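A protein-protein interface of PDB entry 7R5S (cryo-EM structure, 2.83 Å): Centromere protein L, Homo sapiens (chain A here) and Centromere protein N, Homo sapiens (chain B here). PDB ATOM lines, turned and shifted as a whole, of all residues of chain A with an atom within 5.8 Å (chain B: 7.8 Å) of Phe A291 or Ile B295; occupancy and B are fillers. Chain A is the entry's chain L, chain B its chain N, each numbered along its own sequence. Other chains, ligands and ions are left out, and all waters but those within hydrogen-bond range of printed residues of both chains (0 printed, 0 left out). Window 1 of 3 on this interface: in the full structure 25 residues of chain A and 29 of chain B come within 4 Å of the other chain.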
ATOM      1  N   ILE A 252      38.638  -7.896 -24.607  1.00  0.00           N
ATOM      2  CA  ILE A 252      37.347  -7.827 -23.930  1.00  0.00           C
ATOM      3  C   ILE A 252      37.084  -9.158 -23.239  1.00  0.00           C
ATOM      4  O   ILE A 252      37.281 -10.223 -23.834  1.00  0.00           O
ATOM      5  CB  ILE A 252      36.207  -7.490 -24.910  1.00  0.00           C
ATOM      6  CG1 ILE A 252      36.449  -6.126 -25.559  1.00  0.00           C
ATOM      7  CG2 ILE A 252      34.865  -7.505 -24.199  1.00  0.00           C
ATOM      8  CD1 ILE A 252      35.350  -5.693 -26.500  1.00  0.00           C
ATOM      9  N   SER A 253      36.648  -9.096 -21.985  1.00  0.00           N
ATOM     10  CA  SER A 253      36.285 -10.277 -21.217  1.00  0.00           C
ATOM     11  C   SER A 253      34.788 -10.263 -20.936  1.00  0.00           C
ATOM     12  O   SER A 253      34.217  -9.214 -20.622  1.00  0.00           O
ATOM     13  CB  SER A 253      37.065 -10.341 -19.902  1.00  0.00           C
ATOM     14  OG  SER A 253      36.719 -11.496 -19.159  1.00  0.00           O
ATOM     15  N   PHE A 254      34.156 -11.430 -21.050  1.00  0.00           N
ATOM     16  CA  PHE A 254      32.720 -11.573 -20.831  1.00  0.00           C
ATOM     17  C   PHE A 254      32.499 -12.732 -19.870  1.00  0.00           C
ATOM     18  O   PHE A 254      32.673 -13.893 -20.249  1.00  0.00           O
ATOM     19  CB  PHE A 254      31.981 -11.807 -22.150  1.00  0.00           C
ATOM     20  CG  PHE A 254      30.502 -11.548 -22.077  1.00  0.00           C
ATOM     21  CD1 PHE A 254      29.650 -12.470 -21.493  1.00  0.00           C
ATOM     22  CD2 PHE A 254      29.964 -10.387 -22.603  1.00  0.00           C
ATOM     23  CE1 PHE A 254      28.291 -12.235 -21.429  1.00  0.00           C
ATOM     24  CE2 PHE A 254      28.604 -10.148 -22.543  1.00  0.00           C
ATOM     25  CZ  PHE A 254      27.767 -11.073 -21.955  1.00  0.00           C
ATOM     26  N   ALA A 255      32.125 -12.419 -18.633  1.00  0.00           N
ATOM     27  CA  ALA A 255      31.855 -13.420 -17.612  1.00  0.00           C
ATOM     28  C   ALA A 255      30.365 -13.449 -17.306  1.00  0.00           C
ATOM     29  O   ALA A 255      29.704 -12.406 -17.289  1.00  0.00           O
ATOM     30  CB  ALA A 255      32.648 -13.133 -16.335  1.00  0.00           C
ATOM     31  N   CYS A 286      22.755 -14.720 -29.288  1.00  0.00           N
ATOM     32  CA  CYS A 286      22.144 -14.174 -28.079  1.00  0.00           C
ATOM     33  C   CYS A 286      23.126 -13.285 -27.325  1.00  0.00           C
ATOM     34  O   CYS A 286      22.804 -12.145 -26.965  1.00  0.00           O
ATOM     35  CB  CYS A 286      21.643 -15.307 -27.184  1.00  0.00           C
ATOM     36  SG  CYS A 286      20.191 -16.176 -27.820  1.00  0.00           S
ATOM     37  N   LEU A 287      24.341 -13.788 -27.091  1.00  0.00           N
ATOM     38  CA  LEU A 287      25.356 -12.996 -26.403  1.00  0.00           C
ATOM     39  C   LEU A 287      25.770 -11.785 -27.231  1.00  0.00           C
ATOM     40  O   LEU A 287      25.990 -10.698 -26.681  1.00  0.00           O
ATOM     41  CB  LEU A 287      26.571 -13.865 -26.083  1.00  0.00           C
ATOM     42  CG  LEU A 287      26.315 -15.123 -25.253  1.00  0.00           C
ATOM     43  CD1 LEU A 287      27.595 -15.927 -25.096  1.00  0.00           C
ATOM     44  CD2 LEU A 287      25.736 -14.763 -23.895  1.00  0.00           C
ATOM     45  N   TYR A 288      25.885 -11.954 -28.551  1.00  0.00           N
ATOM     46  CA  TYR A 288      26.238 -10.828 -29.412  1.00  0.00           C
ATOM     47  C   TYR A 288      25.220  -9.701 -29.287  1.00  0.00           C
ATOM     48  O   TYR A 288      25.585  -8.528 -29.134  1.00  0.00           O
ATOM     49  CB  TYR A 288      26.350 -11.291 -30.865  1.00  0.00           C
ATOM     50  CG  TYR A 288      27.538 -12.182 -31.146  1.00  0.00           C
ATOM     51  CD1 TYR A 288      28.624 -12.219 -30.283  1.00  0.00           C
ATOM     52  CD2 TYR A 288      27.574 -12.985 -32.279  1.00  0.00           C
ATOM     53  CE1 TYR A 288      29.711 -13.032 -30.539  1.00  0.00           C
ATOM     54  CE2 TYR A 288      28.655 -13.800 -32.542  1.00  0.00           C
ATOM     55  CZ  TYR A 288      29.721 -13.820 -31.669  1.00  0.00           C
ATOM     56  OH  TYR A 288      30.802 -14.631 -31.929  1.00  0.00           O
ATOM     57  N   SER A 289      23.930 -10.042 -29.337  1.00  0.00           N
ATOM     58  CA  SER A 289      22.888  -9.027 -29.238  1.00  0.00           C
ATOM     59  C   SER A 289      22.846  -8.411 -27.845  1.00  0.00           C
ATOM     60  O   SER A 289      22.639  -7.200 -27.705  1.00  0.00           O
ATOM     61  CB  SER A 289      21.532  -9.630 -29.600  1.00  0.00           C
ATOM     62  OG  SER A 289      20.914 -10.211 -28.466  1.00  0.00           O
ATOM     63  N   HIS A 290      23.040  -9.225 -26.803  1.00  0.00           N
ATOM     64  CA  HIS A 290      23.036  -8.687 -25.447  1.00  0.00           C
ATOM     65  C   HIS A 290      24.187  -7.711 -25.236  1.00  0.00           C
ATOM     66  O   HIS A 290      24.046  -6.722 -24.507  1.00  0.00           O
ATOM     67  CB  HIS A 290      23.104  -9.824 -24.428  1.00  0.00           C
ATOM     68  CG  HIS A 290      22.827  -9.390 -23.023  1.00  0.00           C
ATOM     69  ND1 HIS A 290      21.677  -8.721 -22.663  1.00  0.00           N
ATOM     70  CD2 HIS A 290      23.550  -9.531 -21.887  1.00  0.00           C
ATOM     71  CE1 HIS A 290      21.703  -8.467 -21.367  1.00  0.00           C
ATOM     72  NE2 HIS A 290      22.829  -8.948 -20.872  1.00  0.00           N
ATOM     73  N   PHE A 291      25.333  -7.968 -25.869  1.00  0.00           N
ATOM     74  CA  PHE A 291      26.462  -7.051 -25.742  1.00  0.00           C
ATOM     75  C   PHE A 291      26.249  -5.792 -26.574  1.00  0.00           C
ATOM     76  O   PHE A 291      26.595  -4.686 -26.138  1.00  0.00           O
ATOM     77  CB  PHE A 291      27.756  -7.755 -26.149  1.00  0.00           C
ATOM     78  CG  PHE A 291      29.002  -7.010 -25.766  1.00  0.00           C
ATOM     79  CD1 PHE A 291      29.574  -6.095 -26.634  1.00  0.00           C
ATOM     80  CD2 PHE A 291      29.605  -7.228 -24.540  1.00  0.00           C
ATOM     81  CE1 PHE A 291      30.720  -5.410 -26.285  1.00  0.00           C
ATOM     82  CE2 PHE A 291      30.752  -6.546 -24.186  1.00  0.00           C
ATOM     83  CZ  PHE A 291      31.310  -5.636 -25.059  1.00  0.00           C
ATOM     84  N   HIS A 292      25.685  -5.939 -27.776  1.00  0.00           N
ATOM     85  CA  HIS A 292      25.488  -4.783 -28.644  1.00  0.00           C
ATOM     86  C   HIS A 292      24.397  -3.860 -28.118  1.00  0.00           C
ATOM     87  O   HIS A 292      24.457  -2.646 -28.345  1.00  0.00           O
ATOM     88  CB  HIS A 292      25.156  -5.238 -30.064  1.00  0.00           C
ATOM     89  CG  HIS A 292      24.956  -4.109 -31.026  1.00  0.00           C
ATOM     90  ND1 HIS A 292      23.726  -3.530 -31.250  1.00  0.00           N
ATOM     91  CD2 HIS A 292      25.831  -3.450 -31.822  1.00  0.00           C
ATOM     92  CE1 HIS A 292      23.851  -2.564 -32.142  1.00  0.00           C
ATOM     93  NE2 HIS A 292      25.119  -2.495 -32.505  1.00  0.00           N
ATOM     94  N   ARG A 293      23.396  -4.406 -27.423  1.00  0.00           N
ATOM     95  CA  ARG A 293      22.337  -3.562 -26.880  1.00  0.00           C
ATOM     96  C   ARG A 293      22.864  -2.615 -25.812  1.00  0.00           C
ATOM     97  O   ARG A 293      22.270  -1.558 -25.572  1.00  0.00           O
ATOM     98  CB  ARG A 293      21.214  -4.429 -26.310  1.00  0.00           C
ATOM     99  CG  ARG A 293      19.880  -3.711 -26.185  1.00  0.00           C
ATOM    100  CD  ARG A 293      18.979  -4.389 -25.166  1.00  0.00           C
ATOM    101  NE  ARG A 293      19.401  -4.114 -23.797  1.00  0.00           N
ATOM    102  CZ  ARG A 293      18.715  -4.476 -22.717  1.00  0.00           C
ATOM    103  NH1 ARG A 293      17.570  -5.130 -22.845  1.00  0.00           N
ATOM    104  NH2 ARG A 293      19.175  -4.182 -21.509  1.00  0.00           N
ATOM    105  N   HIS A 294      23.972  -2.971 -25.165  1.00  0.00           N
ATOM    106  CA  HIS A 294      24.544  -2.166 -24.093  1.00  0.00           C
ATOM    107  C   HIS A 294      25.718  -1.308 -24.541  1.00  0.00           C
ATOM    108  O   HIS A 294      25.799  -0.138 -24.156  1.00  0.00           O
ATOM    109  CB  HIS A 294      24.991  -3.066 -22.937  1.00  0.00           C
ATOM    110  CG  HIS A 294      23.858  -3.612 -22.124  1.00  0.00           C
ATOM    111  ND1 HIS A 294      23.284  -2.911 -21.085  1.00  0.00           N
ATOM    112  CD2 HIS A 294      23.193  -4.788 -22.198  1.00  0.00           C
ATOM    113  CE1 HIS A 294      22.314  -3.633 -20.553  1.00  0.00           C
ATOM    114  NE2 HIS A 294      22.238  -4.777 -21.210  1.00  0.00           N
ATOM    115  N   PHE A 295      26.632  -1.850 -25.347  1.00  0.00           N
ATOM    116  CA  PHE A 295      27.849  -1.130 -25.695  1.00  0.00           C
ATOM    117  C   PHE A 295      27.929  -0.704 -27.154  1.00  0.00           C
ATOM    118  O   PHE A 295      28.877  -0.001 -27.518  1.00  0.00           O
ATOM    119  CB  PHE A 295      29.081  -1.976 -25.346  1.00  0.00           C
ATOM    120  CG  PHE A 295      29.280  -2.171 -23.873  1.00  0.00           C
ATOM    121  CD1 PHE A 295      29.960  -1.229 -23.121  1.00  0.00           C
ATOM    122  CD2 PHE A 295      28.780  -3.292 -23.236  1.00  0.00           C
ATOM    123  CE1 PHE A 295      30.141  -1.403 -21.765  1.00  0.00           C
ATOM    124  CE2 PHE A 295      28.958  -3.472 -21.879  1.00  0.00           C
ATOM    125  CZ  PHE A 295      29.639  -2.526 -21.143  1.00  0.00           C
ATOM    126  N   LYS A 296      26.968  -1.103 -27.990  1.00  0.00           N
ATOM    127  CA  LYS A 296      26.939  -0.734 -29.408  1.00  0.00           C
ATOM    128  C   LYS A 296      28.209  -1.166 -30.139  1.00  0.00           C
ATOM    129  O   LYS A 296      28.643  -0.513 -31.091  1.00  0.00           O
ATOM    130  CB  LYS A 296      26.709   0.769 -29.591  1.00  0.00           C
ATOM    131  CG  LYS A 296      25.527   1.320 -28.814  1.00  0.00           C
ATOM    132  CD  LYS A 296      24.230   0.647 -29.228  1.00  0.00           C
ATOM    133  CE  LYS A 296      23.056   1.174 -28.421  1.00  0.00           C
ATOM    134  NZ  LYS A 296      21.783   0.496 -28.788  1.00  0.00           N
ATOM    135  N   ILE A 297      28.815  -2.266 -29.701  1.00  0.00           N
ATOM    136  CA  ILE A 297      30.025  -2.806 -30.310  1.00  0.00           C
ATOM    137  C   ILE A 297      29.687  -4.149 -30.938  1.00  0.00           C
ATOM    138  O   ILE A 297      29.107  -5.021 -30.280  1.00  0.00           O
ATOM    139  CB  ILE A 297      31.160  -2.948 -29.281  1.00  0.00           C
ATOM    140  CG1 ILE A 297      31.562  -1.577 -28.736  1.00  0.00           C
ATOM    141  CG2 ILE A 297      32.360  -3.645 -29.901  1.00  0.00           C
ATOM    142  CD1 ILE A 297      32.673  -1.629 -27.714  1.00  0.00           C
ATOM    143  N   LEU A 299      30.378  -7.503 -31.615  1.00  0.00           N
ATOM    144  CA  LEU A 299      31.265  -8.553 -31.132  1.00  0.00           C
ATOM    145  C   LEU A 299      31.478  -9.660 -32.154  1.00  0.00           C
ATOM    146  O   LEU A 299      32.342 -10.518 -31.940  1.00  0.00           O
ATOM    147  CB  LEU A 299      30.711  -9.143 -29.835  1.00  0.00           C
ATOM    148  CG  LEU A 299      31.729  -9.514 -28.757  1.00  0.00           C
ATOM    149  CD1 LEU A 299      32.532  -8.296 -28.338  1.00  0.00           C
ATOM    150  CD2 LEU A 299      31.028 -10.132 -27.559  1.00  0.00           C
ATOM    151  N   PHE B 266      42.452   0.063 -17.819  1.00  0.00           N
ATOM    152  CA  PHE B 266      41.475  -0.901 -17.336  1.00  0.00           C
ATOM    153  C   PHE B 266      40.141  -0.211 -17.099  1.00  0.00           C
ATOM    154  O   PHE B 266      40.090   0.964 -16.725  1.00  0.00           O
ATOM    155  CB  PHE B 266      41.959  -1.582 -16.050  1.00  0.00           C
ATOM    156  CG  PHE B 266      41.043  -2.662 -15.551  1.00  0.00           C
ATOM    157  CD1 PHE B 266      41.082  -3.930 -16.104  1.00  0.00           C
ATOM    158  CD2 PHE B 266      40.151  -2.412 -14.523  1.00  0.00           C
ATOM    159  CE1 PHE B 266      40.244  -4.927 -15.645  1.00  0.00           C
ATOM    160  CE2 PHE B 266      39.311  -3.405 -14.059  1.00  0.00           C
ATOM    161  CZ  PHE B 266      39.357  -4.664 -14.622  1.00  0.00           C
ATOM    162  N   ALA B 267      39.063  -0.958 -17.329  1.00  0.00           N
ATOM    163  CA  ALA B 267      37.715  -0.501 -17.023  1.00  0.00           C
ATOM    164  C   ALA B 267      36.855  -1.714 -16.698  1.00  0.00           C
ATOM    165  O   ALA B 267      37.037  -2.788 -17.274  1.00  0.00           O
ATOM    166  CB  ALA B 267      37.105   0.293 -18.182  1.00  0.00           C
ATOM    167  N   GLN B 268      35.916  -1.537 -15.770  1.00  0.00           N
ATOM    168  CA  GLN B 268      35.098  -2.646 -15.298  1.00  0.00           C
ATOM    169  C   GLN B 268      33.639  -2.225 -15.204  1.00  0.00           C
ATOM    170  O   GLN B 268      33.325  -1.147 -14.692  1.00  0.00           O
ATOM    171  CB  GLN B 268      35.583  -3.152 -13.933  1.00  0.00           C
ATOM    172  CG  GLN B 268      34.750  -4.284 -13.360  1.00  0.00           C
ATOM    173  CD  GLN B 268      35.328  -4.842 -12.076  1.00  0.00           C
ATOM    174  OE1 GLN B 268      36.509  -5.181 -12.010  1.00  0.00           O
ATOM    175  NE2 GLN B 268      34.497  -4.937 -11.046  1.00  0.00           N
ATOM    176  N   TYR B 269      32.753  -3.091 -15.697  1.00  0.00           N
ATOM    177  CA  TYR B 269      31.316  -2.869 -15.665  1.00  0.00           C
ATOM    178  C   TYR B 269      30.626  -4.090 -15.077  1.00  0.00           C
ATOM    179  O   TYR B 269      30.966  -5.230 -15.412  1.00  0.00           O
ATOM    180  CB  TYR B 269      30.756  -2.593 -17.068  1.00  0.00           C
ATOM    181  CG  TYR B 269      31.264  -1.324 -17.712  1.00  0.00           C
ATOM    182  CD1 TYR B 269      32.510  -1.283 -18.324  1.00  0.00           C
ATOM    183  CD2 TYR B 269      30.493  -0.171 -17.720  1.00  0.00           C
ATOM    184  CE1 TYR B 269      32.977  -0.127 -18.917  1.00  0.00           C
ATOM    185  CE2 TYR B 269      30.951   0.990 -18.311  1.00  0.00           C
ATOM    186  CZ  TYR B 269      32.193   1.006 -18.907  1.00  0.00           C
ATOM    187  OH  TYR B 269      32.654   2.160 -19.498  1.00  0.00           O
ATOM    188  N   LYS B 270      29.660  -3.850 -14.198  1.00  0.00           N
ATOM    189  CA  LYS B 270      28.787  -4.890 -13.673  1.00  0.00           C
ATOM    190  C   LYS B 270      27.376  -4.624 -14.175  1.00  0.00           C
ATOM    191  O   LYS B 270      26.911  -3.481 -14.140  1.00  0.00           O
ATOM    192  CB  LYS B 270      28.820  -4.918 -12.143  1.00  0.00           C
ATOM    193  CG  LYS B 270      27.995  -6.031 -11.524  1.00  0.00           C
ATOM    194  CD  LYS B 270      28.111  -6.021 -10.009  1.00  0.00           C
ATOM    195  CE  LYS B 270      27.284  -7.131  -9.385  1.00  0.00           C
ATOM    196  NZ  LYS B 270      27.383  -7.126  -7.899  1.00  0.00           N
ATOM    197  N   LEU B 271      26.705  -5.670 -14.655  1.00  0.00           N
ATOM    198  CA  LEU B 271      25.403  -5.533 -15.292  1.00  0.00           C
ATOM    199  C   LEU B 271      24.400  -6.452 -14.612  1.00  0.00           C
ATOM    200  O   LEU B 271      24.659  -7.650 -14.451  1.00  0.00           O
ATOM    201  CB  LEU B 271      25.483  -5.860 -16.787  1.00  0.00           C
ATOM    202  CG  LEU B 271      26.483  -5.051 -17.615  1.00  0.00           C
ATOM    203  CD1 LEU B 271      26.483  -5.520 -19.060  1.00  0.00           C
ATOM    204  CD2 LEU B 271      26.175  -3.565 -17.530  1.00  0.00           C
ATOM    205  N   PHE B 275      17.282  -9.597 -19.944  1.00  0.00           N
ATOM    206  CA  PHE B 275      17.515  -9.978 -21.330  1.00  0.00           C
ATOM    207  C   PHE B 275      16.256  -9.710 -22.146  1.00  0.00           C
ATOM    208  O   PHE B 275      15.199 -10.289 -21.877  1.00  0.00           O
ATOM    209  CB  PHE B 275      17.916 -11.448 -21.415  1.00  0.00           C
ATOM    210  CG  PHE B 275      18.205 -11.920 -22.811  1.00  0.00           C
ATOM    211  CD1 PHE B 275      19.412 -11.625 -23.420  1.00  0.00           C
ATOM    212  CD2 PHE B 275      17.272 -12.668 -23.510  1.00  0.00           C
ATOM    213  CE1 PHE B 275      19.681 -12.060 -24.703  1.00  0.00           C
ATOM    214  CE2 PHE B 275      17.537 -13.107 -24.794  1.00  0.00           C
ATOM    215  CZ  PHE B 275      18.743 -12.802 -25.390  1.00  0.00           C
ATOM    216  N   CYS B 293      26.112 -10.106 -15.132  1.00  0.00           N
ATOM    217  CA  CYS B 293      27.274 -10.129 -16.010  1.00  0.00           C
ATOM    218  C   CYS B 293      28.358  -9.205 -15.472  1.00  0.00           C
ATOM    219  O   CYS B 293      28.074  -8.217 -14.790  1.00  0.00           O
ATOM    220  CB  CYS B 293      26.906  -9.719 -17.442  1.00  0.00           C
ATOM    221  SG  CYS B 293      25.760 -10.842 -18.274  1.00  0.00           S
ATOM    222  N   LEU B 294      29.605  -9.533 -15.803  1.00  0.00           N
ATOM    223  CA  LEU B 294      30.763  -8.731 -15.420  1.00  0.00           C
ATOM    224  C   LEU B 294      31.685  -8.623 -16.622  1.00  0.00           C
ATOM    225  O   LEU B 294      32.185  -9.639 -17.114  1.00  0.00           O
ATOM    226  CB  LEU B 294      31.499  -9.351 -14.229  1.00  0.00           C
ATOM    227  CG  LEU B 294      32.747  -8.616 -13.738  1.00  0.00           C
ATOM    228  CD1 LEU B 294      32.383  -7.242 -13.201  1.00  0.00           C
ATOM    229  CD2 LEU B 294      33.468  -9.433 -12.680  1.00  0.00           C
ATOM    230  N   ILE B 295      31.914  -7.398 -17.093  1.00  0.00           N
ATOM    231  CA  ILE B 295      32.687  -7.145 -18.302  1.00  0.00           C
ATOM    232  C   ILE B 295      33.902  -6.303 -17.944  1.00  0.00           C
ATOM    233  O   ILE B 295      33.816  -5.389 -17.117  1.00  0.00           O
ATOM    234  CB  ILE B 295      31.825  -6.449 -19.377  1.00  0.00           C
ATOM    235  CG1 ILE B 295      30.557  -7.264 -19.636  1.00  0.00           C
ATOM    236  CG2 ILE B 295      32.611  -6.264 -20.666  1.00  0.00           C
ATOM    237  CD1 ILE B 295      29.669  -6.693 -20.709  1.00  0.00           C
ATOM    238  N   LYS B 296      35.039  -6.619 -18.563  1.00  0.00           N
ATOM    239  CA  LYS B 296      36.294  -5.929 -18.301  1.00  0.00           C
ATOM    240  C   LYS B 296      36.941  -5.527 -19.616  1.00  0.00           C
ATOM    241  O   LYS B 296      37.141  -6.369 -20.497  1.00  0.00           O
ATOM    242  CB  LYS B 296      37.252  -6.810 -17.492  1.00  0.00           C
ATOM    243  CG  LYS B 296      36.723  -7.222 -16.131  1.00  0.00           C
ATOM    244  CD  LYS B 296      37.704  -8.130 -15.411  1.00  0.00           C
ATOM    245  CE  LYS B 296      37.161  -8.566 -14.061  1.00  0.00           C
ATOM    246  NZ  LYS B 296      38.107  -9.467 -13.348  1.00  0.00           N
ATOM    247  N   PHE B 297      37.267  -4.245 -19.742  1.00  0.00           N
ATOM    248  CA  PHE B 297      38.006  -3.720 -20.882  1.00  0.00           C
ATOM    249  C   PHE B 297      39.456  -3.508 -20.474  1.00  0.00           C
ATOM    250  O   PHE B 297      39.732  -2.817 -19.486  1.00  0.00           O
ATOM    251  CB  PHE B 297      37.398  -2.405 -21.373  1.00  0.00           C
ATOM    252  CG  PHE B 297      36.062  -2.561 -22.037  1.00  0.00           C
ATOM    253  CD1 PHE B 297      34.903  -2.636 -21.284  1.00  0.00           C
ATOM    254  CD2 PHE B 297      35.963  -2.623 -23.416  1.00  0.00           C
ATOM    255  CE1 PHE B 297      33.672  -2.776 -21.893  1.00  0.00           C
ATOM    256  CE2 PHE B 297      34.735  -2.762 -24.031  1.00  0.00           C
ATOM    257  CZ  PHE B 297      33.588  -2.839 -23.268  1.00  0.00           C
ATOM    258  N   SER B 298      40.376  -4.100 -21.233  1.00  0.00           N
ATOM    259  CA  SER B 298      41.801  -4.027 -20.952  1.00  0.00           C
ATOM    260  C   SER B 298      42.551  -3.635 -22.215  1.00  0.00           C
ATOM    261  O   SER B 298      42.265  -4.148 -23.301  1.00  0.00           O
ATOM    262  CB  SER B 298      42.330  -5.365 -20.423  1.00  0.00           C
ATOM    263  OG  SER B 298      43.728  -5.475 -20.623  1.00  0.00           O
ATOM    264  N   SER B 320      28.217   4.056 -26.913  1.00  0.00           N
ATOM    265  CA  SER B 320      27.384   4.061 -25.722  1.00  0.00           C
ATOM    266  C   SER B 320      27.915   5.085 -24.721  1.00  0.00           C
ATOM    267  O   SER B 320      29.131   5.256 -24.593  1.00  0.00           O
ATOM    268  CB  SER B 320      27.351   2.673 -25.084  1.00  0.00           C
ATOM    269  OG  SER B 320      26.255   2.546 -24.195  1.00  0.00           O
ATOM    270  N   LEU B 323      30.903   4.338 -22.253  1.00  0.00           N
ATOM    271  CA  LEU B 323      32.300   4.271 -22.661  1.00  0.00           C
ATOM    272  C   LEU B 323      32.922   5.634 -22.928  1.00  0.00           C
ATOM    273  O   LEU B 323      34.153   5.732 -22.984  1.00  0.00           O
ATOM    274  CB  LEU B 323      32.443   3.406 -23.919  1.00  0.00           C
ATOM    275  CG  LEU B 323      32.056   1.932 -23.783  1.00  0.00           C
ATOM    276  CD1 LEU B 323      32.150   1.229 -25.126  1.00  0.00           C
ATOM    277  CD2 LEU B 323      32.933   1.243 -22.754  1.00  0.00           C
ATOM    278  N   ASN B 332      35.817   4.754 -12.948  1.00  0.00           N
ATOM    279  CA  ASN B 332      36.493   3.681 -13.666  1.00  0.00           C
ATOM    280  C   ASN B 332      35.733   2.370 -13.514  1.00  0.00           C
ATOM    281  O   ASN B 332      35.823   1.488 -14.374  1.00  0.00           O
ATOM    282  CB  ASN B 332      37.930   3.529 -13.165  1.00  0.00           C
ATOM    283  CG  ASN B 332      38.853   2.946 -14.213  1.00  0.00           C
ATOM    284  OD1 ASN B 332      38.599   3.059 -15.411  1.00  0.00           O
ATOM    285  ND2 ASN B 332      39.934   2.319 -13.766  1.00  0.00           N
ATOM    286  N   PHE B 334      31.914   0.668 -12.885  1.00  0.00           N
ATOM    287  CA  PHE B 334      30.511   1.002 -13.081  1.00  0.00           C
ATOM    288  C   PHE B 334      29.612  -0.154 -12.663  1.00  0.00           C
ATOM    289  O   PHE B 334      29.968  -1.327 -12.808  1.00  0.00           O
ATOM    290  CB  PHE B 334      30.221   1.360 -14.543  1.00  0.00           C
ATOM    291  CG  PHE B 334      30.907   2.611 -15.011  1.00  0.00           C
ATOM    292  CD1 PHE B 334      32.223   2.577 -15.437  1.00  0.00           C
ATOM    293  CD2 PHE B 334      30.231   3.818 -15.036  1.00  0.00           C
ATOM    294  CE1 PHE B 334      32.854   3.723 -15.872  1.00  0.00           C
ATOM    295  CE2 PHE B 334      30.857   4.969 -15.470  1.00  0.00           C
ATOM    296  CZ  PHE B 334      32.169   4.921 -15.889  1.00  0.00           C
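Of the 17 printed residues of chain A, 9 touch a printed residue of chain B. Hydrophobic or aromatic side chains of chain A within 4 Å of the printed part of chain B: Ile A252, Ala A255, His A290, Phe A291, Phe A295 and Ile A297. Among the printed residues, no Asp or Glu carboxylate lies within 4 Å of a Lys or Arg side-chain nitrogen of the other chain.
The backbone NH (N) of Leu B271 sits at hydrogen-bond distance from the backbone carbonyl oxygen (O) of Cys B293, 2.9 Å away. The backbone NH (N) of Tyr B269 is in hydrogen-bond range of the backbone carbonyl oxygen (O) of Ile B295 (2.9 Å). The backbone carbonyl oxygen of Ala B267 sits at hydrogen-bond distance from the backbone NH of Phe B297. The backbone carbonyl oxygen of Cys A286 sits at hydrogen-bond distance from the side-chain hydroxyl of Ser A289 (3.1 Å). The guanidinium group of Arg A293 is in hydrogen-bond range of a ring nitrogen (NE2) of His A294 (3.1 Å).
Phe A291 touches one residue of chain B. Ile B295 touches three residues of chain A. Of the printed residues of chain B, Ala A255 touches Cys B293 (3.6 Å) and Leu B294 (3.2 Å). Of the printed residues of chain B, His A294 touches Ser B320 (2.7 Å). Printed residues of chain A within 4 Å of Phe B275: Cys A286 (3.9 Å) and His A290 (3.8 Å). Phe B334 touches none of the printed residues of chain A. Phe A254 touches none of the printed residues of chain B. The nearest residue of chain A that does not touch Ile B295 is Phe A254 (4.1 Å).
The backbone NH (N) of Ser A253 is in hydrogen-bond range of the backbone carbonyl oxygen (O) of Lys B296, 3.1 Å away. The backbone carbonyl oxygen (O) of His A294 is in hydrogen-bond range of the side-chain hydroxyl (OG) of Ser B320 (2.7 Å). The backbone carbonyl oxygen (O) of Leu B294 is in hydrogen-bond range of the backbone NH (N) of Ala A255.
Lys B296 touches Ile A252. Phe B297 touches Ile A252. O of Ser A253 touches CG2 of Ile B295, 3.4 Å away. CE1 of Phe B275 touches O of Cys A286 (3.9 Å). Phe B275 touches His A290 (CD1 to ND1, 3.8 Å). Phe A291 touches Ile B295. Phe A295 touches Ile B295. CE1 of Phe B297 touches CE1 of Phe A295 (3.8 Å). Phe A295 touches Ser B320 (CA to CB, 3.9 Å). Leu B323 touches Ile A297.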
